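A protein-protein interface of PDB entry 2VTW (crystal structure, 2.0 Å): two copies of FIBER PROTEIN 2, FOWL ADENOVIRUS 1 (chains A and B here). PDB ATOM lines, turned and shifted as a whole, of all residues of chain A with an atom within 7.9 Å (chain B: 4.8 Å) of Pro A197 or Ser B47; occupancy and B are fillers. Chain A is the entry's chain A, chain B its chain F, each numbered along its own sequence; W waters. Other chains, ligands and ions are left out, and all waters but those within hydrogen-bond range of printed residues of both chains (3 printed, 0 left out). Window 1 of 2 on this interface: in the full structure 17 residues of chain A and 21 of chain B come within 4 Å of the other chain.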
ATOM      1  N   ASN A  39      24.618   4.168  11.547  1.00  0.00           N
ATOM      2  CA  ASN A  39      23.301   3.867  12.118  1.00  0.00           C
ATOM      3  C   ASN A  39      23.215   2.367  12.048  1.00  0.00           C
ATOM      4  O   ASN A  39      23.287   1.803  10.958  1.00  0.00           O
ATOM      5  CB  ASN A  39      22.149   4.506  11.332  1.00  0.00           C
ATOM      6  CG  ASN A  39      20.741   4.236  11.949  1.00  0.00           C
ATOM      7  OD1 ASN A  39      20.497   3.220  12.569  1.00  0.00           O
ATOM      8  ND2 ASN A  39      19.821   5.133  11.710  1.00  0.00           N
ATOM      9  N   GLY A  42      18.825   1.658  14.229  1.00  0.00           N
ATOM     10  CA  GLY A  42      18.219   2.712  15.042  1.00  0.00           C
ATOM     11  C   GLY A  42      19.052   3.279  16.179  1.00  0.00           C
ATOM     12  O   GLY A  42      18.542   4.079  16.942  1.00  0.00           O
ATOM     13  N   MET A  43      20.326   2.883  16.267  1.00  0.00           N
ATOM     14  CA  MET A  43      21.292   3.446  17.222  1.00  0.00           C
ATOM     15  C   MET A  43      22.385   4.163  16.455  1.00  0.00           C
ATOM     16  O   MET A  43      23.044   3.570  15.601  1.00  0.00           O
ATOM     17  CB  MET A  43      21.933   2.334  18.087  1.00  0.00           C
ATOM     18  CG  MET A  43      22.718   2.861  19.328  1.00  0.00           C
ATOM     19  SD  MET A  43      21.595   3.529  20.602  1.00  0.00           S
ATOM     20  CE  MET A  43      20.772   2.031  21.126  1.00  0.00           C
ATOM     21  N   LEU A  44      22.587   5.431  16.787  1.00  0.00           N
ATOM     22  CA  LEU A  44      23.521   6.299  16.111  1.00  0.00           C
ATOM     23  C   LEU A  44      24.844   6.407  16.867  1.00  0.00           C
ATOM     24  O   LEU A  44      24.872   6.852  18.012  1.00  0.00           O
ATOM     25  CB  LEU A  44      22.903   7.701  15.995  1.00  0.00           C
ATOM     26  CG  LEU A  44      23.631   8.724  15.118  1.00  0.00           C
ATOM     27  CD1 LEU A  44      23.638   8.273  13.591  1.00  0.00           C
ATOM     28  CD2 LEU A  44      22.993  10.082  15.319  1.00  0.00           C
ATOM     29  N   THR A  45      25.931   6.039  16.198  1.00  0.00           N
ATOM     30  CA  THR A  45      27.298   6.224  16.720  1.00  0.00           C
ATOM     31  C   THR A  45      27.989   7.250  15.827  1.00  0.00           C
ATOM     32  O   THR A  45      28.027   7.072  14.618  1.00  0.00           O
ATOM     33  CB  THR A  45      28.118   4.920  16.690  1.00  0.00           C
ATOM     34  OG1 THR A  45      27.519   3.950  17.544  1.00  0.00           O
ATOM     35  CG2 THR A  45      29.546   5.172  17.155  1.00  0.00           C
ATOM     36  N   PHE A 103      20.511   9.522   9.747  1.00  0.00           N
ATOM     37  CA  PHE A 103      21.464  10.028  10.729  1.00  0.00           C
ATOM     38  C   PHE A 103      20.905  11.101  11.646  1.00  0.00           C
ATOM     39  O   PHE A 103      21.639  11.710  12.432  1.00  0.00           O
ATOM     40  CB  PHE A 103      22.753  10.447  10.007  1.00  0.00           C
ATOM     41  CG  PHE A 103      23.270   9.370   9.171  1.00  0.00           C
ATOM     42  CD1 PHE A 103      23.999   8.318   9.737  1.00  0.00           C
ATOM     43  CD2 PHE A 103      22.914   9.286   7.831  1.00  0.00           C
ATOM     44  CE1 PHE A 103      24.413   7.261   8.963  1.00  0.00           C
ATOM     45  CE2 PHE A 103      23.326   8.213   7.057  1.00  0.00           C
ATOM     46  CZ  PHE A 103      24.073   7.194   7.626  1.00  0.00           C
ATOM     47  N   GLU A 104      19.587  11.290  11.576  1.00  0.00           N
ATOM     48  CA  GLU A 104      18.891  12.164  12.480  1.00  0.00           C
ATOM     49  C   GLU A 104      18.794  11.468  13.831  1.00  0.00           C
ATOM     50  O   GLU A 104      18.322  10.339  13.910  1.00  0.00           O
ATOM     51  CB  GLU A 104      17.483  12.446  11.981  1.00  0.00           C
ATOM     52  CG  GLU A 104      16.724  13.472  12.807  1.00  0.00           C
ATOM     53  CD  GLU A 104      15.233  13.573  12.424  1.00  0.00           C
ATOM     54  OE1 GLU A 104      14.839  13.033  11.353  1.00  0.00           O
ATOM     55  OE2 GLU A 104      14.491  14.228  13.199  1.00  0.00           O
ATOM     56  N   PRO A 105      19.224  12.158  14.894  1.00  0.00           N
ATOM     57  CA  PRO A 105      19.054  11.593  16.232  1.00  0.00           C
ATOM     58  C   PRO A 105      17.602  11.681  16.695  1.00  0.00           C
ATOM     59  O   PRO A 105      16.879  12.621  16.318  1.00  0.00           O
ATOM     60  CB  PRO A 105      19.938  12.485  17.077  1.00  0.00           C
ATOM     61  CG  PRO A 105      19.881  13.832  16.354  1.00  0.00           C
ATOM     62  CD  PRO A 105      19.890  13.471  14.921  1.00  0.00           C
ATOM     63  N   ALA A 106      17.169  10.709  17.495  1.00  0.00           N
ATOM     64  CA  ALA A 106      15.827  10.745  18.066  1.00  0.00           C
ATOM     65  C   ALA A 106      15.629  11.967  18.929  1.00  0.00           C
ATOM     66  O   ALA A 106      16.577  12.539  19.460  1.00  0.00           O
ATOM     67  CB  ALA A 106      15.520   9.426  18.863  1.00  0.00           C
ATOM     68  N   ARG A 107      14.381  12.391  19.066  1.00  0.00           N
ATOM     69  CA  ARG A 107      14.017  13.468  19.971  1.00  0.00           C
ATOM     70  C   ARG A 107      14.569  13.076  21.326  1.00  0.00           C
ATOM     71  O   ARG A 107      14.450  11.924  21.709  1.00  0.00           O
ATOM     72  CB  ARG A 107      12.481  13.571  20.061  1.00  0.00           C
ATOM     73  CG  ARG A 107      11.894  14.814  20.776  1.00  0.00           C
ATOM     74  CD  ARG A 107      10.390  14.578  21.241  1.00  0.00           C
ATOM     75  NE  ARG A 107      10.290  14.440  22.719  1.00  0.00           N
ATOM     76  CZ  ARG A 107       9.668  13.464  23.387  1.00  0.00           C
ATOM     77  NH1 ARG A 107       9.019  12.488  22.768  1.00  0.00           N
ATOM     78  NH2 ARG A 107       9.675  13.473  24.707  1.00  0.00           N
ATOM     79  N   ASN A 108      15.140  14.040  22.022  1.00  0.00           N
ATOM     80  CA  ASN A 108      15.689  13.853  23.357  1.00  0.00           C
ATOM     81  C   ASN A 108      14.597  14.054  24.424  1.00  0.00           C
ATOM     82  O   ASN A 108      14.178  15.183  24.700  1.00  0.00           O
ATOM     83  CB  ASN A 108      16.855  14.826  23.553  1.00  0.00           C
ATOM     84  CG  ASN A 108      17.606  14.581  24.842  1.00  0.00           C
ATOM     85  OD1 ASN A 108      17.242  13.694  25.624  1.00  0.00           O
ATOM     86  ND2 ASN A 108      18.667  15.346  25.064  1.00  0.00           N
ATOM     87  N   PRO A 109      14.152  12.969  25.048  1.00  0.00           N
ATOM     88  CA  PRO A 109      13.040  13.089  25.983  1.00  0.00           C
ATOM     89  C   PRO A 109      13.322  13.781  27.331  1.00  0.00           C
ATOM     90  O   PRO A 109      12.387  14.098  28.055  1.00  0.00           O
ATOM     91  CB  PRO A 109      12.623  11.647  26.186  1.00  0.00           C
ATOM     92  CG  PRO A 109      13.858  10.890  26.025  1.00  0.00           C
ATOM     93  CD  PRO A 109      14.632  11.588  24.963  1.00  0.00           C
ATOM     94  N   VAL A 153      21.908  15.809  22.455  1.00  0.00           N
ATOM     95  CA  VAL A 153      20.917  15.938  21.377  1.00  0.00           C
ATOM     96  C   VAL A 153      19.930  17.051  21.785  1.00  0.00           C
ATOM     97  O   VAL A 153      19.388  17.051  22.891  1.00  0.00           O
ATOM     98  CB  VAL A 153      20.196  14.639  21.125  1.00  0.00           C
ATOM     99  CG1 VAL A 153      18.997  14.851  20.188  1.00  0.00           C
ATOM    100  CG2 VAL A 153      21.163  13.627  20.552  1.00  0.00           C
ATOM    101  N   ILE A 167      22.874  17.191  17.250  1.00  0.00           N
ATOM    102  CA  ILE A 167      23.787  16.933  18.376  1.00  0.00           C
ATOM    103  C   ILE A 167      24.745  18.116  18.620  1.00  0.00           C
ATOM    104  O   ILE A 167      25.531  18.443  17.760  1.00  0.00           O
ATOM    105  CB  ILE A 167      24.646  15.621  18.168  1.00  0.00           C
ATOM    106  CG1 ILE A 167      23.796  14.481  17.595  1.00  0.00           C
ATOM    107  CG2 ILE A 167      25.345  15.233  19.526  1.00  0.00           C
ATOM    108  CD1 ILE A 167      24.566  13.328  16.983  1.00  0.00           C
ATOM    109  N   HIS A 194      30.299   9.534  20.274  1.00  0.00           N
ATOM    110  CA  HIS A 194      29.006   9.719  20.921  1.00  0.00           C
ATOM    111  C   HIS A 194      28.073   8.651  20.438  1.00  0.00           C
ATOM    112  O   HIS A 194      28.068   8.346  19.258  1.00  0.00           O
ATOM    113  CB  HIS A 194      28.422  11.073  20.538  1.00  0.00           C
ATOM    114  CG  HIS A 194      27.104  11.354  21.171  1.00  0.00           C
ATOM    115  ND1 HIS A 194      25.945  11.471  20.440  1.00  0.00           N
ATOM    116  CD2 HIS A 194      26.747  11.490  22.472  1.00  0.00           C
ATOM    117  CE1 HIS A 194      24.940  11.717  21.257  1.00  0.00           C
ATOM    118  NE2 HIS A 194      25.397  11.728  22.495  1.00  0.00           N
ATOM    119  N   THR A 195      27.276   8.079  21.348  1.00  0.00           N
ATOM    120  CA  THR A 195      26.215   7.157  20.971  1.00  0.00           C
ATOM    121  C   THR A 195      24.862   7.674  21.482  1.00  0.00           C
ATOM    122  O   THR A 195      24.730   8.195  22.598  1.00  0.00           O
ATOM    123  CB  THR A 195      26.490   5.704  21.462  1.00  0.00           C
ATOM    124  OG1 THR A 195      27.715   5.234  20.916  1.00  0.00           O
ATOM    125  CG2 THR A 195      25.392   4.734  21.028  1.00  0.00           C
ATOM    126  N   CYS A 196      23.853   7.554  20.625  1.00  0.00           N
ATOM    127  CA  CYS A 196      22.488   7.924  20.998  1.00  0.00           C
ATOM    128  C   CYS A 196      21.513   7.187  20.091  1.00  0.00           C
ATOM    129  O   CYS A 196      21.911   6.658  19.044  1.00  0.00           O
ATOM    130  CB  CYS A 196      22.269   9.439  20.966  1.00  0.00           C
ATOM    131  SG  CYS A 196      22.283  10.226  19.323  1.00  0.00           S
ATOM    132  N   PRO A 197      20.248   7.081  20.531  1.00  0.00           N
ATOM    133  CA  PRO A 197      19.203   6.605  19.664  1.00  0.00           C
ATOM    134  C   PRO A 197      18.997   7.506  18.456  1.00  0.00           C
ATOM    135  O   PRO A 197      18.974   8.722  18.572  1.00  0.00           O
ATOM    136  CB  PRO A 197      17.965   6.619  20.569  1.00  0.00           C
ATOM    137  CG  PRO A 197      18.526   6.498  21.960  1.00  0.00           C
ATOM    138  CD  PRO A 197      19.743   7.346  21.892  1.00  0.00           C
ATOM    139  N   ALA A 198      18.857   6.858  17.309  1.00  0.00           N
ATOM    140  CA  ALA A 198      18.465   7.476  16.054  1.00  0.00           C
ATOM    141  C   ALA A 198      16.944   7.543  15.984  1.00  0.00           C
ATOM    142  O   ALA A 198      16.276   6.680  16.525  1.00  0.00           O
ATOM    143  CB  ALA A 198      18.999   6.629  14.894  1.00  0.00           C
ATOM    144  N   ALA A 199      16.416   8.550  15.282  1.00  0.00           N
ATOM    145  CA  ALA A 199      14.964   8.669  14.979  1.00  0.00           C
ATOM    146  C   ALA A 199      14.409   7.432  14.292  1.00  0.00           C
ATOM    147  O   ALA A 199      13.277   7.055  14.525  1.00  0.00           O
ATOM    148  CB  ALA A 199      14.695   9.903  14.124  1.00  0.00           C
ATOM    149  N   ARG A 200      15.200   6.766  13.471  1.00  0.00           N
ATOM    150  CA  ARG A 200      14.703   5.587  12.754  1.00  0.00           C
ATOM    151  C   ARG A 200      15.844   4.680  12.339  1.00  0.00           C
ATOM    152  O   ARG A 200      16.979   5.125  12.292  1.00  0.00           O
ATOM    153  CB  ARG A 200      13.933   6.044  11.491  1.00  0.00           C
ATOM    154  CG  ARG A 200      14.766   6.912  10.563  1.00  0.00           C
ATOM    155  CD  ARG A 200      13.954   7.573   9.501  1.00  0.00           C
ATOM    156  NE  ARG A 200      12.999   8.528  10.056  1.00  0.00           N
ATOM    157  CZ  ARG A 200      13.283   9.750  10.486  1.00  0.00           C
ATOM    158  NH1 ARG A 200      14.502  10.267  10.429  1.00  0.00           N
ATOM    159  NH2 ARG A 200      12.313  10.498  10.945  1.00  0.00           N
ATOM    160  N   PHE B  34      13.196   4.434  29.493  1.00  0.00           N
ATOM    161  CA  PHE B  34      13.145   4.093  28.089  1.00  0.00           C
ATOM    162  C   PHE B  34      14.452   3.399  27.733  1.00  0.00           C
ATOM    163  O   PHE B  34      15.524   3.983  27.831  1.00  0.00           O
ATOM    164  CB  PHE B  34      12.882   5.330  27.222  1.00  0.00           C
ATOM    165  CG  PHE B  34      12.473   4.997  25.804  1.00  0.00           C
ATOM    166  CD1 PHE B  34      11.473   4.068  25.558  1.00  0.00           C
ATOM    167  CD2 PHE B  34      13.075   5.605  24.740  1.00  0.00           C
ATOM    168  CE1 PHE B  34      11.114   3.748  24.283  1.00  0.00           C
ATOM    169  CE2 PHE B  34      12.718   5.298  23.437  1.00  0.00           C
ATOM    170  CZ  PHE B  34      11.728   4.357  23.205  1.00  0.00           C
ATOM    171  N   LEU B  35      14.330   2.136  27.352  1.00  0.00           N
ATOM    172  CA  LEU B  35      15.433   1.256  27.123  1.00  0.00           C
ATOM    173  C   LEU B  35      15.452   0.835  25.651  1.00  0.00           C
ATOM    174  O   LEU B  35      14.486   0.255  25.150  1.00  0.00           O
ATOM    175  CB  LEU B  35      15.299   0.025  28.022  1.00  0.00           C
ATOM    176  CG  LEU B  35      16.266  -1.128  27.809  1.00  0.00           C
ATOM    177  CD1 LEU B  35      17.695  -0.661  28.173  1.00  0.00           C
ATOM    178  CD2 LEU B  35      15.798  -2.401  28.581  1.00  0.00           C
ATOM    179  N   GLN B  36      16.569   1.116  24.983  1.00  0.00           N
ATOM    180  CA  GLN B  36      16.802   0.686  23.615  1.00  0.00           C
ATOM    181  C   GLN B  36      18.156  -0.002  23.531  1.00  0.00           C
ATOM    182  O   GLN B  36      19.196   0.559  23.887  1.00  0.00           O
ATOM    183  CB  GLN B  36      16.767   1.898  22.691  1.00  0.00           C
ATOM    184  CG  GLN B  36      15.418   2.604  22.682  1.00  0.00           C
ATOM    185  CD  GLN B  36      15.450   3.919  21.926  1.00  0.00           C
ATOM    186  OE1 GLN B  36      15.864   4.946  22.467  1.00  0.00           O
ATOM    187  NE2 GLN B  36      14.934   3.906  20.680  1.00  0.00           N
ATOM    188  N   THR B  45      24.924  -3.128  22.941  1.00  0.00           N
ATOM    189  CA  THR B  45      24.879  -1.712  23.313  1.00  0.00           C
ATOM    190  C   THR B  45      23.519  -1.394  23.937  1.00  0.00           C
ATOM    191  O   THR B  45      22.478  -1.793  23.391  1.00  0.00           O
ATOM    192  CB  THR B  45      25.092  -0.798  22.097  1.00  0.00           C
ATOM    193  OG1 THR B  45      26.397  -1.058  21.565  1.00  0.00           O
ATOM    194  CG2 THR B  45      24.928   0.715  22.465  1.00  0.00           C
ATOM    195  N   THR B  46      23.543  -0.676  25.070  1.00  0.00           N
ATOM    196  CA  THR B  46      22.351  -0.334  25.847  1.00  0.00           C
ATOM    197  C   THR B  46      22.254   1.164  25.985  1.00  0.00           C
ATOM    198  O   THR B  46      23.167   1.815  26.486  1.00  0.00           O
ATOM    199  CB  THR B  46      22.363  -1.037  27.226  1.00  0.00           C
ATOM    200  OG1 THR B  46      22.367  -2.462  27.038  1.00  0.00           O
ATOM    201  CG2 THR B  46      21.133  -0.626  28.100  1.00  0.00           C
ATOM    202  N   SER B  47      21.148   1.728  25.516  1.00  0.00           N
ATOM    203  CA  SER B  47      20.778   3.103  25.771  1.00  0.00           C
ATOM    204  C   SER B  47      19.611   3.141  26.783  1.00  0.00           C
ATOM    205  O   SER B  47      18.571   2.510  26.567  1.00  0.00           O
ATOM    206  CB  SER B  47      20.346   3.792  24.465  1.00  0.00           C
ATOM    207  OG  SER B  47      20.084   5.157  24.669  1.00  0.00           O
ATOM    208  N   LEU B  48      19.794   3.888  27.876  1.00  0.00           N
ATOM    209  CA  LEU B  48      18.838   3.941  28.962  1.00  0.00           C
ATOM    210  C   LEU B  48      18.569   5.377  29.374  1.00  0.00           C
ATOM    211  O   LEU B  48      19.493   6.156  29.612  1.00  0.00           O
ATOM    212  CB  LEU B  48      19.354   3.142  30.159  1.00  0.00           C
ATOM    213  CG  LEU B  48      18.431   3.176  31.372  1.00  0.00           C
ATOM    214  CD1 LEU B  48      17.079   2.503  31.049  1.00  0.00           C
ATOM    215  CD2 LEU B  48      19.115   2.568  32.561  1.00  0.00           C
ATOM    216  N   TYR B  49      17.286   5.745  29.402  1.00  0.00           N
ATOM    217  CA  TYR B  49      16.837   6.989  30.013  1.00  0.00           C
ATOM    218  C   TYR B  49      16.054   6.581  31.239  1.00  0.00           C
ATOM    219  O   TYR B  49      15.331   5.607  31.208  1.00  0.00           O
ATOM    220  CB  TYR B  49      15.876   7.762  29.116  1.00  0.00           C
ATOM    221  CG  TYR B  49      16.433   8.343  27.843  1.00  0.00           C
ATOM    222  CD1 TYR B  49      17.016   9.591  27.844  1.00  0.00           C
ATOM    223  CD2 TYR B  49      16.322   7.674  26.631  1.00  0.00           C
ATOM    224  CE1 TYR B  49      17.526  10.152  26.698  1.00  0.00           C
ATOM    225  CE2 TYR B  49      16.808   8.246  25.452  1.00  0.00           C
ATOM    226  CZ  TYR B  49      17.416   9.486  25.502  1.00  0.00           C
ATOM    227  OH  TYR B  49      17.900  10.100  24.364  1.00  0.00           O
ATOM    228  N   PRO B 191      20.837  10.249  27.381  1.00  0.00           N
ATOM    229  CA  PRO B 191      20.898   8.786  27.289  1.00  0.00           C
ATOM    230  C   PRO B 191      22.177   8.233  27.943  1.00  0.00           C
ATOM    231  O   PRO B 191      23.276   8.729  27.667  1.00  0.00           O
ATOM    232  CB  PRO B 191      20.918   8.540  25.775  1.00  0.00           C
ATOM    233  CG  PRO B 191      21.594   9.709  25.212  1.00  0.00           C
ATOM    234  CD  PRO B 191      21.091  10.885  26.074  1.00  0.00           C
ATOM    235  N   VAL B 192      22.007   7.260  28.836  1.00  0.00           N
ATOM    236  CA  VAL B 192      23.105   6.540  29.477  1.00  0.00           C
ATOM    237  C   VAL B 192      23.419   5.340  28.604  1.00  0.00           C
ATOM    238  O   VAL B 192      22.612   4.423  28.503  1.00  0.00           O
ATOM    239  CB  VAL B 192      22.733   6.096  30.944  1.00  0.00           C
ATOM    240  CG1 VAL B 192      23.917   5.409  31.625  1.00  0.00           C
ATOM    241  CG2 VAL B 192      22.195   7.281  31.767  1.00  0.00           C
ATOM    242  N   VAL B 193      24.579   5.364  27.945  1.00  0.00           N
ATOM    243  CA  VAL B 193      24.947   4.312  27.034  1.00  0.00           C
ATOM    244  C   VAL B 193      26.077   3.413  27.601  1.00  0.00           C
ATOM    245  O   VAL B 193      27.092   3.891  28.110  1.00  0.00           O
ATOM    246  CB  VAL B 193      25.336   4.886  25.631  1.00  0.00           C
ATOM    247  CG1 VAL B 193      25.610   3.779  24.660  1.00  0.00           C
ATOM    248  CG2 VAL B 193      24.230   5.788  25.113  1.00  0.00           C
HETATM  249  O   HOH W   1      15.960   3.852  17.570  1.00  0.00           O
HETATM  250  O   HOH W   2      16.394   9.515  22.323  1.00  0.00           O
HETATM  251  O   HOH W   3      14.320   6.190  18.680  1.00  0.00           O
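ND2 of Asn A108 lies within hydrogen-bond range of O of Val A153 (2.9 Å). The backbone carbonyl oxygen (O) of Phe B34 sits at hydrogen-bond distance from the backbone NH (N) of Tyr B49 (2.9 Å). The backbone NH of Ala A106 sits at hydrogen-bond distance from the backbone carbonyl oxygen of Pro A197. The backbone carbonyl oxygen of Gln B36 lies within hydrogen-bond range of the backbone NH of Ser B47.
Pro A197 touches two residues of chain B. Printed residues of chain B within 4 Å of Asn A108: Tyr B49 (3.7 Å). Printed residues of chain B within 4 Å of Thr A195: Val B193 (3.5 Å). Of the printed residues of chain A, Val B193 touches Thr A195. The nearest residue of chain B that does not touch Pro A197 is Tyr B49 (4.1 Å). The nearest residue of chain A that does not touch Ser B47 is Cys A196 (5.2 Å). The nearest printed residue of chain B that does not touch Thr A195 is Thr B45 (4.3 Å).
Position printed for both chains: 45.
Printed residues of chain B that touch a printed residue of chain A: Gln B36, Ser B47, Tyr B49 and Val B193. Of the 21 printed residues of chain A, 5 touch a printed residue of chain B. Hydrophobic or aromatic side chains of chain A that line the printed part of chain B: Met A43, Pro A109 and Pro A197. Among the printed residues, 7 pairs touch across the chains. Among the printed residues, no Asp or Glu carboxylate lies within 4 Å of a Lys or Arg side-chain nitrogen of the other chain.
Among the printed residues, merely in contact across the chains: Met A43 with Gln B36, Met A43 with Ser B47, Asn A108 with Tyr B49, Pro A109 with Tyr B49, Thr A195 with Val B193, Pro A197 with Gln B36 and Pro A197 with Ser B47.
Water W2 bridges OH of Tyr B49 (2.6 Å) and O of Arg A107 (3.2 Å). Water W1 lies within hydrogen-bond range of O of Gly A42 (2.7 Å), O of Ala A198 (3.0 Å) and NE2 of Gln B36 (3.3 Å). Water W3 lies within hydrogen-bond range of O of Ala A198 (3.0 Å) and NE2 of Gln B36 (3.1 Å).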
